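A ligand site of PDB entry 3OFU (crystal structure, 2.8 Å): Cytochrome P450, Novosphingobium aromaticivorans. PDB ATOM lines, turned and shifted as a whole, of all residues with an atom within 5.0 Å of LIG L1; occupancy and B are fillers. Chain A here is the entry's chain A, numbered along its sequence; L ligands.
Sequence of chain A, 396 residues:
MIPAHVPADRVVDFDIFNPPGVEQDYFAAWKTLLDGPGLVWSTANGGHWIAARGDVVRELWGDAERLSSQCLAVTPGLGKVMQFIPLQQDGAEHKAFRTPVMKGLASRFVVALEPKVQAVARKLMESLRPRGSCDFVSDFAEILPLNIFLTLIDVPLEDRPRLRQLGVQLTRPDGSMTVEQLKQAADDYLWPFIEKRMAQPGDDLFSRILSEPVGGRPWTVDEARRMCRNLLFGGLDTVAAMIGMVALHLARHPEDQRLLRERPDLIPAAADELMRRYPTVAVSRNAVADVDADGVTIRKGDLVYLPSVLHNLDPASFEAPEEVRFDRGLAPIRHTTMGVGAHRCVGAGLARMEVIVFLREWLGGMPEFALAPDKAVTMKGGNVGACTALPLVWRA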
ATOM      1  N   TRP A  61      23.130 -36.374   2.336  1.00  0.00           N
ATOM      2  CA  TRP A  61      22.135 -35.366   2.639  1.00  0.00           C
ATOM      3  C   TRP A  61      20.781 -36.008   2.451  1.00  0.00           C
ATOM      4  O   TRP A  61      19.799 -35.621   3.070  1.00  0.00           O
ATOM      5  CB  TRP A  61      22.344 -34.170   1.726  1.00  0.00           C
ATOM      6  CG  TRP A  61      21.612 -32.921   2.129  1.00  0.00           C
ATOM      7  CD1 TRP A  61      20.332 -32.799   2.544  1.00  0.00           C
ATOM      8  CD2 TRP A  61      22.126 -31.598   1.996  1.00  0.00           C
ATOM      9  NE1 TRP A  61      20.025 -31.471   2.721  1.00  0.00           N
ATOM     10  CE2 TRP A  61      21.126 -30.730   2.419  1.00  0.00           C
ATOM     11  CE3 TRP A  61      23.368 -31.060   1.587  1.00  0.00           C
ATOM     12  CZ2 TRP A  61      21.324 -29.364   2.454  1.00  0.00           C
ATOM     13  CZ3 TRP A  61      23.575 -29.700   1.675  1.00  0.00           C
ATOM     14  CH2 TRP A  61      22.583 -28.859   2.074  1.00  0.00           C
ATOM     15  N   SER A  69      18.762 -34.616  11.912  1.00  0.00           N
ATOM     16  CA  SER A  69      18.818 -33.283  11.716  1.00  0.00           C
ATOM     17  C   SER A  69      18.647 -32.711  13.084  1.00  0.00           C
ATOM     18  O   SER A  69      17.977 -31.685  13.261  1.00  0.00           O
ATOM     19  CB  SER A  69      17.644 -32.892  10.822  1.00  0.00           C
ATOM     20  OG  SER A  69      17.883 -33.228   9.473  1.00  0.00           O
ATOM     21  N   ILE A  85      10.738 -26.482  14.035  1.00  0.00           N
ATOM     22  CA  ILE A  85       9.859 -27.422  13.383  1.00  0.00           C
ATOM     23  C   ILE A  85       9.570 -26.934  11.986  1.00  0.00           C
ATOM     24  O   ILE A  85       9.160 -25.738  11.829  1.00  0.00           O
ATOM     25  CB  ILE A  85       8.549 -27.595  14.122  1.00  0.00           C
ATOM     26  CG1 ILE A  85       8.768 -28.516  15.342  1.00  0.00           C
ATOM     27  CG2 ILE A  85       7.389 -28.145  13.211  1.00  0.00           C
ATOM     28  CD1 ILE A  85       7.657 -28.484  16.247  1.00  0.00           C
ATOM     29  N   PRO A  86       9.757 -27.758  10.932  1.00  0.00           N
ATOM     30  CA  PRO A  86      10.127 -29.138  10.857  1.00  0.00           C
ATOM     31  C   PRO A  86      11.577 -29.432  10.820  1.00  0.00           C
ATOM     32  O   PRO A  86      11.910 -30.625  10.861  1.00  0.00           O
ATOM     33  CB  PRO A  86       9.586 -29.582   9.475  1.00  0.00           C
ATOM     34  CG  PRO A  86       9.200 -28.402   8.755  1.00  0.00           C
ATOM     35  CD  PRO A  86       9.543 -27.193   9.583  1.00  0.00           C
ATOM     36  N   LEU A  87      12.438 -28.394  10.730  1.00  0.00           N
ATOM     37  CA  LEU A  87      13.753 -28.535  10.198  1.00  0.00           C
ATOM     38  C   LEU A  87      14.523 -29.438  10.997  1.00  0.00           C
ATOM     39  O   LEU A  87      15.408 -30.052  10.490  1.00  0.00           O
ATOM     40  CB  LEU A  87      14.420 -27.137  10.003  1.00  0.00           C
ATOM     41  CG  LEU A  87      15.963 -27.317   9.839  1.00  0.00           C
ATOM     42  CD1 LEU A  87      16.424 -27.724   8.336  1.00  0.00           C
ATOM     43  CD2 LEU A  87      16.842 -26.249  10.482  1.00  0.00           C
ATOM     44  N   HIS A  94       8.614 -35.932  11.762  1.00  0.00           N
ATOM     45  CA  HIS A  94       8.952 -34.985  10.758  1.00  0.00           C
ATOM     46  C   HIS A  94       7.963 -35.122   9.609  1.00  0.00           C
ATOM     47  O   HIS A  94       7.368 -34.103   9.137  1.00  0.00           O
ATOM     48  CB  HIS A  94      10.456 -35.132  10.334  1.00  0.00           C
ATOM     49  CG  HIS A  94      10.745 -34.576   8.965  1.00  0.00           C
ATOM     50  ND1 HIS A  94      10.876 -33.208   8.744  1.00  0.00           N
ATOM     51  CD2 HIS A  94      10.780 -35.171   7.745  1.00  0.00           C
ATOM     52  CE1 HIS A  94      10.973 -32.977   7.449  1.00  0.00           C
ATOM     53  NE2 HIS A  94      10.930 -34.152   6.825  1.00  0.00           N
ATOM     54  N   ARG A  98       5.697 -31.821   8.579  1.00  0.00           N
ATOM     55  CA  ARG A  98       6.007 -31.290   7.235  1.00  0.00           C
ATOM     56  C   ARG A  98       4.776 -31.136   6.364  1.00  0.00           C
ATOM     57  O   ARG A  98       4.567 -29.985   5.857  1.00  0.00           O
ATOM     58  CB  ARG A  98       7.167 -32.046   6.471  1.00  0.00           C
ATOM     59  CG  ARG A  98       7.222 -31.615   4.938  1.00  0.00           C
ATOM     60  CD  ARG A  98       8.137 -32.450   3.964  1.00  0.00           C
ATOM     61  NE  ARG A  98       9.358 -31.694   3.882  1.00  0.00           N
ATOM     62  CZ  ARG A  98       9.761 -30.990   2.839  1.00  0.00           C
ATOM     63  NH1 ARG A  98       9.131 -31.001   1.694  1.00  0.00           N
ATOM     64  NH2 ARG A  98      10.905 -30.340   2.954  1.00  0.00           N
ATOM     65  N   LEU A 105       2.684 -23.710   2.009  1.00  0.00           N
ATOM     66  CA  LEU A 105       3.422 -23.076   1.048  1.00  0.00           C
ATOM     67  C   LEU A 105       3.155 -23.579  -0.448  1.00  0.00           C
ATOM     68  O   LEU A 105       3.976 -23.238  -1.370  1.00  0.00           O
ATOM     69  CB  LEU A 105       4.844 -23.273   1.474  1.00  0.00           C
ATOM     70  CG  LEU A 105       5.403 -22.278   2.494  1.00  0.00           C
ATOM     71  CD1 LEU A 105       6.498 -22.862   3.517  1.00  0.00           C
ATOM     72  CD2 LEU A 105       5.943 -21.141   1.798  1.00  0.00           C
ATOM     73  N   LEU A 152       3.743 -12.007   3.959  1.00  0.00           N
ATOM     74  CA  LEU A 152       3.266 -13.409   3.920  1.00  0.00           C
ATOM     75  C   LEU A 152       2.227 -13.671   5.078  1.00  0.00           C
ATOM     76  O   LEU A 152       1.289 -14.531   4.921  1.00  0.00           O
ATOM     77  CB  LEU A 152       4.364 -14.459   4.113  1.00  0.00           C
ATOM     78  CG  LEU A 152       5.610 -14.406   3.264  1.00  0.00           C
ATOM     79  CD1 LEU A 152       6.580 -15.529   3.610  1.00  0.00           C
ATOM     80  CD2 LEU A 152       5.174 -14.436   1.826  1.00  0.00           C
ATOM     81  N   LEU A 205      -0.130 -16.953   5.524  1.00  0.00           N
ATOM     82  CA  LEU A 205       0.694 -18.094   5.613  1.00  0.00           C
ATOM     83  C   LEU A 205       0.466 -18.876   6.864  1.00  0.00           C
ATOM     84  O   LEU A 205       0.230 -20.077   6.803  1.00  0.00           O
ATOM     85  CB  LEU A 205       2.167 -17.677   5.555  1.00  0.00           C
ATOM     86  CG  LEU A 205       3.190 -18.870   5.712  1.00  0.00           C
ATOM     87  CD1 LEU A 205       3.089 -19.938   4.573  1.00  0.00           C
ATOM     88  CD2 LEU A 205       4.638 -18.372   5.962  1.00  0.00           C
ATOM     89  N   ASN A 230      10.954 -21.080  12.888  1.00  0.00           N
ATOM     90  CA  ASN A 230      11.473 -21.745  11.736  1.00  0.00           C
ATOM     91  C   ASN A 230      11.092 -21.132  10.325  1.00  0.00           C
ATOM     92  O   ASN A 230      11.972 -21.002   9.429  1.00  0.00           O
ATOM     93  CB  ASN A 230      11.239 -23.308  11.878  1.00  0.00           C
ATOM     94  CG  ASN A 230      11.940 -24.120  10.806  1.00  0.00           C
ATOM     95  OD1 ASN A 230      12.767 -23.575   9.976  1.00  0.00           O
ATOM     96  ND2 ASN A 230      11.623 -25.389  10.739  1.00  0.00           N
ATOM     97  N   LEU A 231       9.831 -20.801  10.105  1.00  0.00           N
ATOM     98  CA  LEU A 231       9.505 -20.019   8.938  1.00  0.00           C
ATOM     99  C   LEU A 231      10.152 -18.659   8.887  1.00  0.00           C
ATOM    100  O   LEU A 231      10.656 -18.300   7.896  1.00  0.00           O
ATOM    101  CB  LEU A 231       8.020 -19.772   8.901  1.00  0.00           C
ATOM    102  CG  LEU A 231       7.303 -20.918   8.245  1.00  0.00           C
ATOM    103  CD1 LEU A 231       5.951 -20.524   8.180  1.00  0.00           C
ATOM    104  CD2 LEU A 231       7.906 -21.056   6.876  1.00  0.00           C
ATOM    105  N   GLY A 234      14.055 -19.336   8.510  1.00  0.00           N
ATOM    106  CA  GLY A 234      14.290 -20.045   7.240  1.00  0.00           C
ATOM    107  C   GLY A 234      14.126 -19.084   6.073  1.00  0.00           C
ATOM    108  O   GLY A 234      14.630 -19.325   4.967  1.00  0.00           O
ATOM    109  N   GLY A 235      13.444 -17.975   6.289  1.00  0.00           N
ATOM    110  CA  GLY A 235      13.138 -17.072   5.176  1.00  0.00           C
ATOM    111  C   GLY A 235      13.986 -15.822   4.998  1.00  0.00           C
ATOM    112  O   GLY A 235      13.830 -15.127   3.980  1.00  0.00           O
ATOM    113  N   THR A 238      18.752 -16.833   4.357  1.00  0.00           N
ATOM    114  CA  THR A 238      19.019 -17.481   3.072  1.00  0.00           C
ATOM    115  C   THR A 238      18.557 -16.594   1.927  1.00  0.00           C
ATOM    116  O   THR A 238      19.343 -16.299   0.993  1.00  0.00           O
ATOM    117  CB  THR A 238      18.269 -18.822   2.921  1.00  0.00           C
ATOM    118  OG1 THR A 238      16.904 -18.517   3.090  1.00  0.00           O
ATOM    119  CG2 THR A 238      18.588 -19.745   3.943  1.00  0.00           C
ATOM    120  N   VAL A 239      17.306 -16.158   1.948  1.00  0.00           N
ATOM    121  CA  VAL A 239      16.864 -15.254   0.868  1.00  0.00           C
ATOM    122  C   VAL A 239      17.833 -14.054   0.579  1.00  0.00           C
ATOM    123  O   VAL A 239      18.202 -13.821  -0.540  1.00  0.00           O
ATOM    124  CB  VAL A 239      15.410 -14.755   1.159  1.00  0.00           C
ATOM    125  CG1 VAL A 239      14.989 -13.640   0.210  1.00  0.00           C
ATOM    126  CG2 VAL A 239      14.464 -15.931   1.128  1.00  0.00           C
ATOM    127  N   MET A 242      21.081 -15.090  -1.060  1.00  0.00           N
ATOM    128  CA  MET A 242      20.739 -15.285  -2.430  1.00  0.00           C
ATOM    129  C   MET A 242      20.521 -13.934  -3.191  1.00  0.00           C
ATOM    130  O   MET A 242      21.155 -13.757  -4.284  1.00  0.00           O
ATOM    131  CB  MET A 242      19.510 -16.269  -2.528  1.00  0.00           C
ATOM    132  CG  MET A 242      19.073 -16.581  -3.896  1.00  0.00           C
ATOM    133  SD  MET A 242      20.400 -17.341  -4.890  1.00  0.00           S
ATOM    134  CE  MET A 242      20.497 -18.964  -4.040  1.00  0.00           C
ATOM    135  N   VAL A 281      24.215 -22.355   1.285  1.00  0.00           N
ATOM    136  CA  VAL A 281      23.771 -22.946   2.490  1.00  0.00           C
ATOM    137  C   VAL A 281      24.534 -24.225   2.869  1.00  0.00           C
ATOM    138  O   VAL A 281      24.959 -24.962   2.033  1.00  0.00           O
ATOM    139  CB  VAL A 281      22.184 -23.193   2.470  1.00  0.00           C
ATOM    140  CG1 VAL A 281      21.669 -23.984   3.827  1.00  0.00           C
ATOM    141  CG2 VAL A 281      21.301 -21.841   2.291  1.00  0.00           C
ATOM    142  N   VAL A 283      24.515 -27.691   5.890  1.00  0.00           N
ATOM    143  CA  VAL A 283      23.873 -28.163   7.016  1.00  0.00           C
ATOM    144  C   VAL A 283      24.666 -29.258   7.788  1.00  0.00           C
ATOM    145  O   VAL A 283      25.631 -29.934   7.234  1.00  0.00           O
ATOM    146  CB  VAL A 283      22.531 -28.738   6.656  1.00  0.00           C
ATOM    147  CG1 VAL A 283      21.588 -27.692   6.245  1.00  0.00           C
ATOM    148  CG2 VAL A 283      22.633 -29.915   5.688  1.00  0.00           C
ATOM    149  N   ARG A 285      24.523 -32.763  10.268  1.00  0.00           N
ATOM    150  CA  ARG A 285      23.751 -33.847  10.709  1.00  0.00           C
ATOM    151  C   ARG A 285      24.474 -34.538  11.874  1.00  0.00           C
ATOM    152  O   ARG A 285      25.755 -34.423  12.032  1.00  0.00           O
ATOM    153  CB  ARG A 285      23.619 -34.803   9.540  1.00  0.00           C
ATOM    154  CG  ARG A 285      22.895 -34.176   8.364  1.00  0.00           C
ATOM    155  CD  ARG A 285      21.469 -34.055   8.709  1.00  0.00           C
ATOM    156  NE  ARG A 285      20.669 -33.723   7.567  1.00  0.00           N
ATOM    157  CZ  ARG A 285      20.306 -32.500   7.213  1.00  0.00           C
ATOM    158  NH1 ARG A 285      20.646 -31.532   7.949  1.00  0.00           N
ATOM    159  NH2 ARG A 285      19.570 -32.305   6.083  1.00  0.00           N
ATOM    160  N   THR A 336      21.451 -29.096  -5.280  1.00  0.00           N
ATOM    161  CA  THR A 336      21.232 -29.067  -3.804  1.00  0.00           C
ATOM    162  C   THR A 336      21.120 -27.670  -3.097  1.00  0.00           C
ATOM    163  O   THR A 336      21.562 -27.434  -1.939  1.00  0.00           O
ATOM    164  CB  THR A 336      22.383 -29.781  -3.110  1.00  0.00           C
ATOM    165  OG1 THR A 336      22.832 -30.902  -3.911  1.00  0.00           O
ATOM    166  CG2 THR A 336      21.854 -30.319  -1.769  1.00  0.00           C
ATOM    167  N   THR A 337      20.697 -26.689  -3.821  1.00  0.00           N
ATOM    168  CA  THR A 337      20.637 -25.429  -3.207  1.00  0.00           C
ATOM    169  C   THR A 337      19.634 -25.535  -2.063  1.00  0.00           C
ATOM    170  O   THR A 337      19.989 -25.295  -0.945  1.00  0.00           O
ATOM    171  CB  THR A 337      20.208 -24.329  -4.203  1.00  0.00           C
ATOM    172  OG1 THR A 337      21.265 -24.270  -5.160  1.00  0.00           O
ATOM    173  CG2 THR A 337      20.025 -23.023  -3.518  1.00  0.00           C
ATOM    174  N   MET A 338      18.396 -25.934  -2.360  1.00  0.00           N
ATOM    175  CA  MET A 338      17.348 -25.976  -1.378  1.00  0.00           C
ATOM    176  C   MET A 338      17.378 -27.339  -0.622  1.00  0.00           C
ATOM    177  O   MET A 338      16.426 -27.713   0.057  1.00  0.00           O
ATOM    178  CB  MET A 338      15.993 -25.778  -2.093  1.00  0.00           C
ATOM    179  CG  MET A 338      15.916 -24.739  -3.108  1.00  0.00           C
ATOM    180  SD  MET A 338      16.149 -22.987  -2.448  1.00  0.00           S
ATOM    181  CE  MET A 338      15.024 -23.304  -1.066  1.00  0.00           C
ATOM    182  N   GLY A 339      18.462 -28.071  -0.784  1.00  0.00           N
ATOM    183  CA  GLY A 339      18.662 -29.304  -0.079  1.00  0.00           C
ATOM    184  C   GLY A 339      18.393 -30.480  -0.909  1.00  0.00           C
ATOM    185  O   GLY A 339      18.579 -30.381  -2.059  1.00  0.00           O
ATOM    186  N   ALA A 342      13.831 -35.818   2.147  1.00  0.00           N
ATOM    187  CA  ALA A 342      12.757 -35.414   3.011  1.00  0.00           C
ATOM    188  C   ALA A 342      12.905 -33.929   3.474  1.00  0.00           C
ATOM    189  O   ALA A 342      11.894 -33.276   3.798  1.00  0.00           O
ATOM    190  CB  ALA A 342      12.672 -36.417   4.287  1.00  0.00           C
ATOM    191  N   HIS A 343      14.152 -33.428   3.651  1.00  0.00           N
ATOM    192  CA  HIS A 343      14.253 -32.119   4.296  1.00  0.00           C
ATOM    193  C   HIS A 343      14.265 -30.869   3.378  1.00  0.00           C
ATOM    194  O   HIS A 343      14.600 -29.760   3.867  1.00  0.00           O
ATOM    195  CB  HIS A 343      15.364 -32.094   5.300  1.00  0.00           C
ATOM    196  CG  HIS A 343      15.029 -32.779   6.592  1.00  0.00           C
ATOM    197  ND1 HIS A 343      14.164 -32.236   7.534  1.00  0.00           N
ATOM    198  CD2 HIS A 343      15.451 -33.956   7.102  1.00  0.00           C
ATOM    199  CE1 HIS A 343      14.057 -33.067   8.556  1.00  0.00           C
ATOM    200  NE2 HIS A 343      14.839 -34.115   8.324  1.00  0.00           N
ATOM    201  N   ARG A 344      13.861 -31.053   2.101  1.00  0.00           N
ATOM    202  CA  ARG A 344      14.128 -30.133   1.033  1.00  0.00           C
ATOM    203  C   ARG A 344      13.263 -28.855   1.077  1.00  0.00           C
ATOM    204  O   ARG A 344      12.045 -28.916   1.040  1.00  0.00           O
ATOM    205  CB  ARG A 344      13.978 -30.843  -0.320  1.00  0.00           C
ATOM    206  CG  ARG A 344      14.141 -29.842  -1.502  1.00  0.00           C
ATOM    207  CD  ARG A 344      14.215 -30.512  -2.853  1.00  0.00           C
ATOM    208  NE  ARG A 344      14.760 -29.516  -3.738  1.00  0.00           N
ATOM    209  CZ  ARG A 344      14.012 -28.830  -4.566  1.00  0.00           C
ATOM    210  NH1 ARG A 344      12.683 -29.037  -4.601  1.00  0.00           N
ATOM    211  NH2 ARG A 344      14.585 -27.908  -5.304  1.00  0.00           N
ATOM    212  N   CYS A 345      13.866 -27.709   1.092  1.00  0.00           N
ATOM    213  CA  CYS A 345      13.132 -26.505   1.414  1.00  0.00           C
ATOM    214  C   CYS A 345      11.704 -26.491   0.974  1.00  0.00           C
ATOM    215  O   CYS A 345      11.378 -26.547  -0.272  1.00  0.00           O
ATOM    216  CB  CYS A 345      13.871 -25.311   0.848  1.00  0.00           C
ATOM    217  SG  CYS A 345      13.496 -23.793   1.656  1.00  0.00           S
ATOM    218  N   VAL A 346      10.788 -26.409   1.957  1.00  0.00           N
ATOM    219  CA  VAL A 346       9.279 -26.163   1.743  1.00  0.00           C
ATOM    220  C   VAL A 346       9.067 -24.909   0.958  1.00  0.00           C
ATOM    221  O   VAL A 346       8.220 -24.842   0.134  1.00  0.00           O
ATOM    222  CB  VAL A 346       8.459 -26.116   3.083  1.00  0.00           C
ATOM    223  CG1 VAL A 346       8.169 -27.530   3.569  1.00  0.00           C
ATOM    224  CG2 VAL A 346       9.187 -25.380   4.157  1.00  0.00           C
ATOM    225  N   GLY A 347       9.922 -23.928   1.217  1.00  0.00           N
ATOM    226  CA  GLY A 347       9.988 -22.661   0.583  1.00  0.00           C
ATOM    227  C   GLY A 347      10.691 -22.522  -0.776  1.00  0.00           C
ATOM    228  O   GLY A 347      10.831 -21.352  -1.317  1.00  0.00           O
ATOM    229  N   LEU A 350       8.489 -20.728  -3.417  1.00  0.00           N
ATOM    230  CA  LEU A 350       8.479 -19.309  -2.937  1.00  0.00           C
ATOM    231  C   LEU A 350       9.761 -18.523  -3.104  1.00  0.00           C
ATOM    232  O   LEU A 350       9.717 -17.359  -3.515  1.00  0.00           O
ATOM    233  CB  LEU A 350       8.140 -19.270  -1.443  1.00  0.00           C
ATOM    234  CG  LEU A 350       8.390 -18.045  -0.637  1.00  0.00           C
ATOM    235  CD1 LEU A 350       7.522 -17.029  -1.200  1.00  0.00           C
ATOM    236  CD2 LEU A 350       7.922 -18.403   0.753  1.00  0.00           C
ATOM    237  N   ALA A 351      10.889 -19.172  -2.747  1.00  0.00           N
ATOM    238  CA  ALA A 351      12.154 -18.528  -2.960  1.00  0.00           C
ATOM    239  C   ALA A 351      12.250 -18.190  -4.460  1.00  0.00           C
ATOM    240  O   ALA A 351      12.602 -17.068  -4.820  1.00  0.00           O
ATOM    241  CB  ALA A 351      13.281 -19.416  -2.483  1.00  0.00           C
ATOM    242  N   GLU A 354      10.431 -15.457  -5.308  1.00  0.00           N
ATOM    243  CA  GLU A 354      11.039 -14.346  -4.729  1.00  0.00           C
ATOM    244  C   GLU A 354      12.096 -13.792  -5.655  1.00  0.00           C
ATOM    245  O   GLU A 354      12.100 -12.558  -5.980  1.00  0.00           O
ATOM    246  CB  GLU A 354      11.535 -14.631  -3.337  1.00  0.00           C
ATOM    247  CG  GLU A 354      10.560 -14.213  -2.197  1.00  0.00           C
ATOM    248  CD  GLU A 354      10.985 -14.826  -0.932  1.00  0.00           C
ATOM    249  OE1 GLU A 354      10.772 -14.355   0.198  1.00  0.00           O
ATOM    250  OE2 GLU A 354      11.637 -15.842  -1.078  1.00  0.00           O
HETATM  251  C1  LIG L   1      14.734 -25.982   4.389  1.00  0.00           C
HETATM  252  C2  LIG L   1      17.664 -23.236   1.866  1.00  0.00           C
HETATM  253  C3  LIG L   1      14.046 -20.146   1.574  1.00  0.00           C
HETATM  254  C4  LIG L   1      11.718 -22.245   5.263  1.00  0.00           C
HETATM  255  C5  LIG L   1      15.776 -25.545   3.685  1.00  0.00           C
HETATM  256  C6  LIG L   1      16.934 -26.392   3.312  1.00  0.00           C
HETATM  257  C7  LIG L   1      17.730 -25.606   2.558  1.00  0.00           C
HETATM  258  C8  LIG L   1      17.107 -24.298   2.487  1.00  0.00           C
HETATM  259  C9  LIG L   1      19.112 -26.027   1.957  1.00  0.00           C
HETATM  260  C10 LIG L   1      17.194 -27.856   3.678  1.00  0.00           C
HETATM  261  C11 LIG L   1      17.801 -27.780   5.008  1.00  0.00           C
HETATM  262  C12 LIG L   1      18.208 -29.156   5.543  1.00  0.00           C
HETATM  263  O1  LIG L   1      18.836 -29.233   6.674  1.00  0.00           O
HETATM  264  O2  LIG L   1      17.982 -30.230   4.928  1.00  0.00           O
HETATM  265  C13 LIG L   1      16.928 -22.163   1.518  1.00  0.00           C
HETATM  266  C14 LIG L   1      17.325 -21.211   0.545  1.00  0.00           C
HETATM  267  C15 LIG L   1      16.245 -20.385   0.474  1.00  0.00           C
HETATM  268  C16 LIG L   1      15.233 -20.809   1.392  1.00  0.00           C
HETATM  269  C17 LIG L   1      18.642 -21.196  -0.219  1.00  0.00           C
HETATM  270  C18 LIG L   1      16.040 -19.138  -0.406  1.00  0.00           C
HETATM  271  C19 LIG L   1      17.057 -18.236  -0.425  1.00  0.00           C
HETATM  272  C20 LIG L   1      13.107 -20.432   2.541  1.00  0.00           C
HETATM  273  C21 LIG L   1      11.864 -19.702   2.700  1.00  0.00           C
HETATM  274  C22 LIG L   1      11.259 -20.318   3.728  1.00  0.00           C
HETATM  275  C23 LIG L   1      12.064 -21.389   4.224  1.00  0.00           C
HETATM  276  C24 LIG L   1      11.419 -18.524   1.756  1.00  0.00           C
HETATM  277  C25 LIG L   1       9.838 -20.079   4.363  1.00  0.00           C
HETATM  278  C26 LIG L   1       9.290 -18.865   4.480  1.00  0.00           C
HETATM  279  C27 LIG L   1      12.315 -23.517   5.359  1.00  0.00           C
HETATM  280  C28 LIG L   1      11.935 -24.608   6.310  1.00  0.00           C
HETATM  281  C29 LIG L   1      12.854 -25.824   5.960  1.00  0.00           C
HETATM  282  C30 LIG L   1      13.769 -25.285   4.936  1.00  0.00           C
HETATM  283  C31 LIG L   1      10.829 -24.675   7.417  1.00  0.00           C
HETATM  284  C32 LIG L   1      12.846 -27.176   6.665  1.00  0.00           C
HETATM  285  C33 LIG L   1      12.109 -28.253   5.948  1.00  0.00           C
HETATM  286  C34 LIG L   1      12.014 -29.704   6.594  1.00  0.00           C
HETATM  287  O3  LIG L   1      12.813 -30.228   7.414  1.00  0.00           O
HETATM  288  O4  LIG L   1      11.106 -30.462   6.197  1.00  0.00           O
HETATM  289  N1  LIG L   1      15.890 -24.338   3.114  1.00  0.00           N
HETATM  290  N2  LIG L   1      15.679 -21.897   2.030  1.00  0.00           N
HETATM  291  N3  LIG L   1      13.189 -21.438   3.439  1.00  0.00           N
HETATM  292  N4  LIG L   1      13.412 -24.027   4.558  1.00  0.00           N
HETATM  293 FE1  LIG L   1      14.545 -23.027   3.209  1.00  0.00          FE
HETATM  294  C1  LG2 L   2      20.408 -23.156   8.963  1.00  0.00           C
HETATM  295  O1  LG2 L   2      19.839 -19.096  13.721  1.00  0.00           O
HETATM  296  C2  LG2 L   2      19.688 -24.157   8.016  1.00  0.00           C
HETATM  297  C3  LG2 L   2      18.644 -23.538   7.025  1.00  0.00           C
HETATM  298  C4  LG2 L   2      18.291 -22.061   7.385  1.00  0.00           C
HETATM  299  C5  LG2 L   2      18.390 -21.729   8.922  1.00  0.00           C
HETATM  300  C6  LG2 L   2      19.431 -22.158   9.702  1.00  0.00           C
HETATM  301  C7  LG2 L   2      19.695 -21.768  11.181  1.00  0.00           C
HETATM  302  C8  LG2 L   2      19.896 -20.508  11.719  1.00  0.00           C
HETATM  303  C9  LG2 L   2      20.248 -20.101  13.177  1.00  0.00           C
HETATM  304  C10 LG2 L   2      21.274 -23.833  10.055  1.00  0.00           C
HETATM  305  C11 LG2 L   2      21.315 -22.372   7.999  1.00  0.00           C
HETATM  306  C12 LG2 L   2      17.264 -20.950   9.524  1.00  0.00           C
HETATM  307  C13 LG2 L   2      21.188 -20.936  13.978  1.00  0.00           C
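An oxygen (O2) of LIG L1 lies within salt-bridge range of the guanidinium group (NH2) of Arg 285 (2.9 Å). ND1 of His 343 sits at hydrogen-bond distance from O3 of LIG L1. NE1 of Trp 61 sits at hydrogen-bond distance from O2 of LIG L1, 3.3 Å away. NE of Arg 98 lies within salt-bridge range of O4 of LIG L1 (3.2 Å). FE1 of LIG L1 is bound by SG of Cys 345 (2.0 Å).
The side-chain hydroxyl of Ser 69 lies within hydrogen-bond range of a ring nitrogen (NE2) of His 343, 3.4 Å away. The side-chain hydroxyl (OG) of Ser 69 sits close to the guanidinium group (NE) of Arg 285, 3.4 Å away. A ring nitrogen (ND1) of His 94 is in hydrogen-bond range of the backbone carbonyl oxygen (O) of Pro 86, at 3.5 Å. The backbone NH (N) of Leu 87 lies close to the side-chain amide nitrogen (ND2) of Asn 230 (3.1 Å). ND2 of Asn 230 lies within hydrogen-bond range of O of Ile 85 (2.7 Å). The backbone carbonyl oxygen of Ala 342 sits at hydrogen-bond distance from the guanidinium group of Arg 98, at 3.0 Å. O of Arg 344 lies within hydrogen-bond range of NH2 of Arg 98. The backbone NH of Cys 345 sits at hydrogen-bond distance from the backbone carbonyl oxygen of Met 338, 2.8 Å away.
The backbone carbonyl oxygen (O) of Gly 234 lies close to a nitrogen (N3) of LIG L1. Merely in contact with LIG L1: His 94, Thr 337, Val 239, Val 283, Thr 238, Leu 87, Leu 231, Met 338, Asn 230, Ala 351, Gly 339, Pro 86, Val 346, Leu 350, Val 281, Ala 342, Met 242, Gly 235 and Glu 354. 25 residues have an atom within 4 Å of LIG L1: Trp 61, Pro 86, Leu 87, His 94, Arg 98, Asn 230, Leu 231, Gly 234, Gly 235, Thr 238, Val 239, Met 242, Val 281, Val 283, Arg 285, Thr 337, Met 338, Gly 339, Ala 342, His 343, Cys 345, Val 346, Leu 350, Ala 351 and Glu 354.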
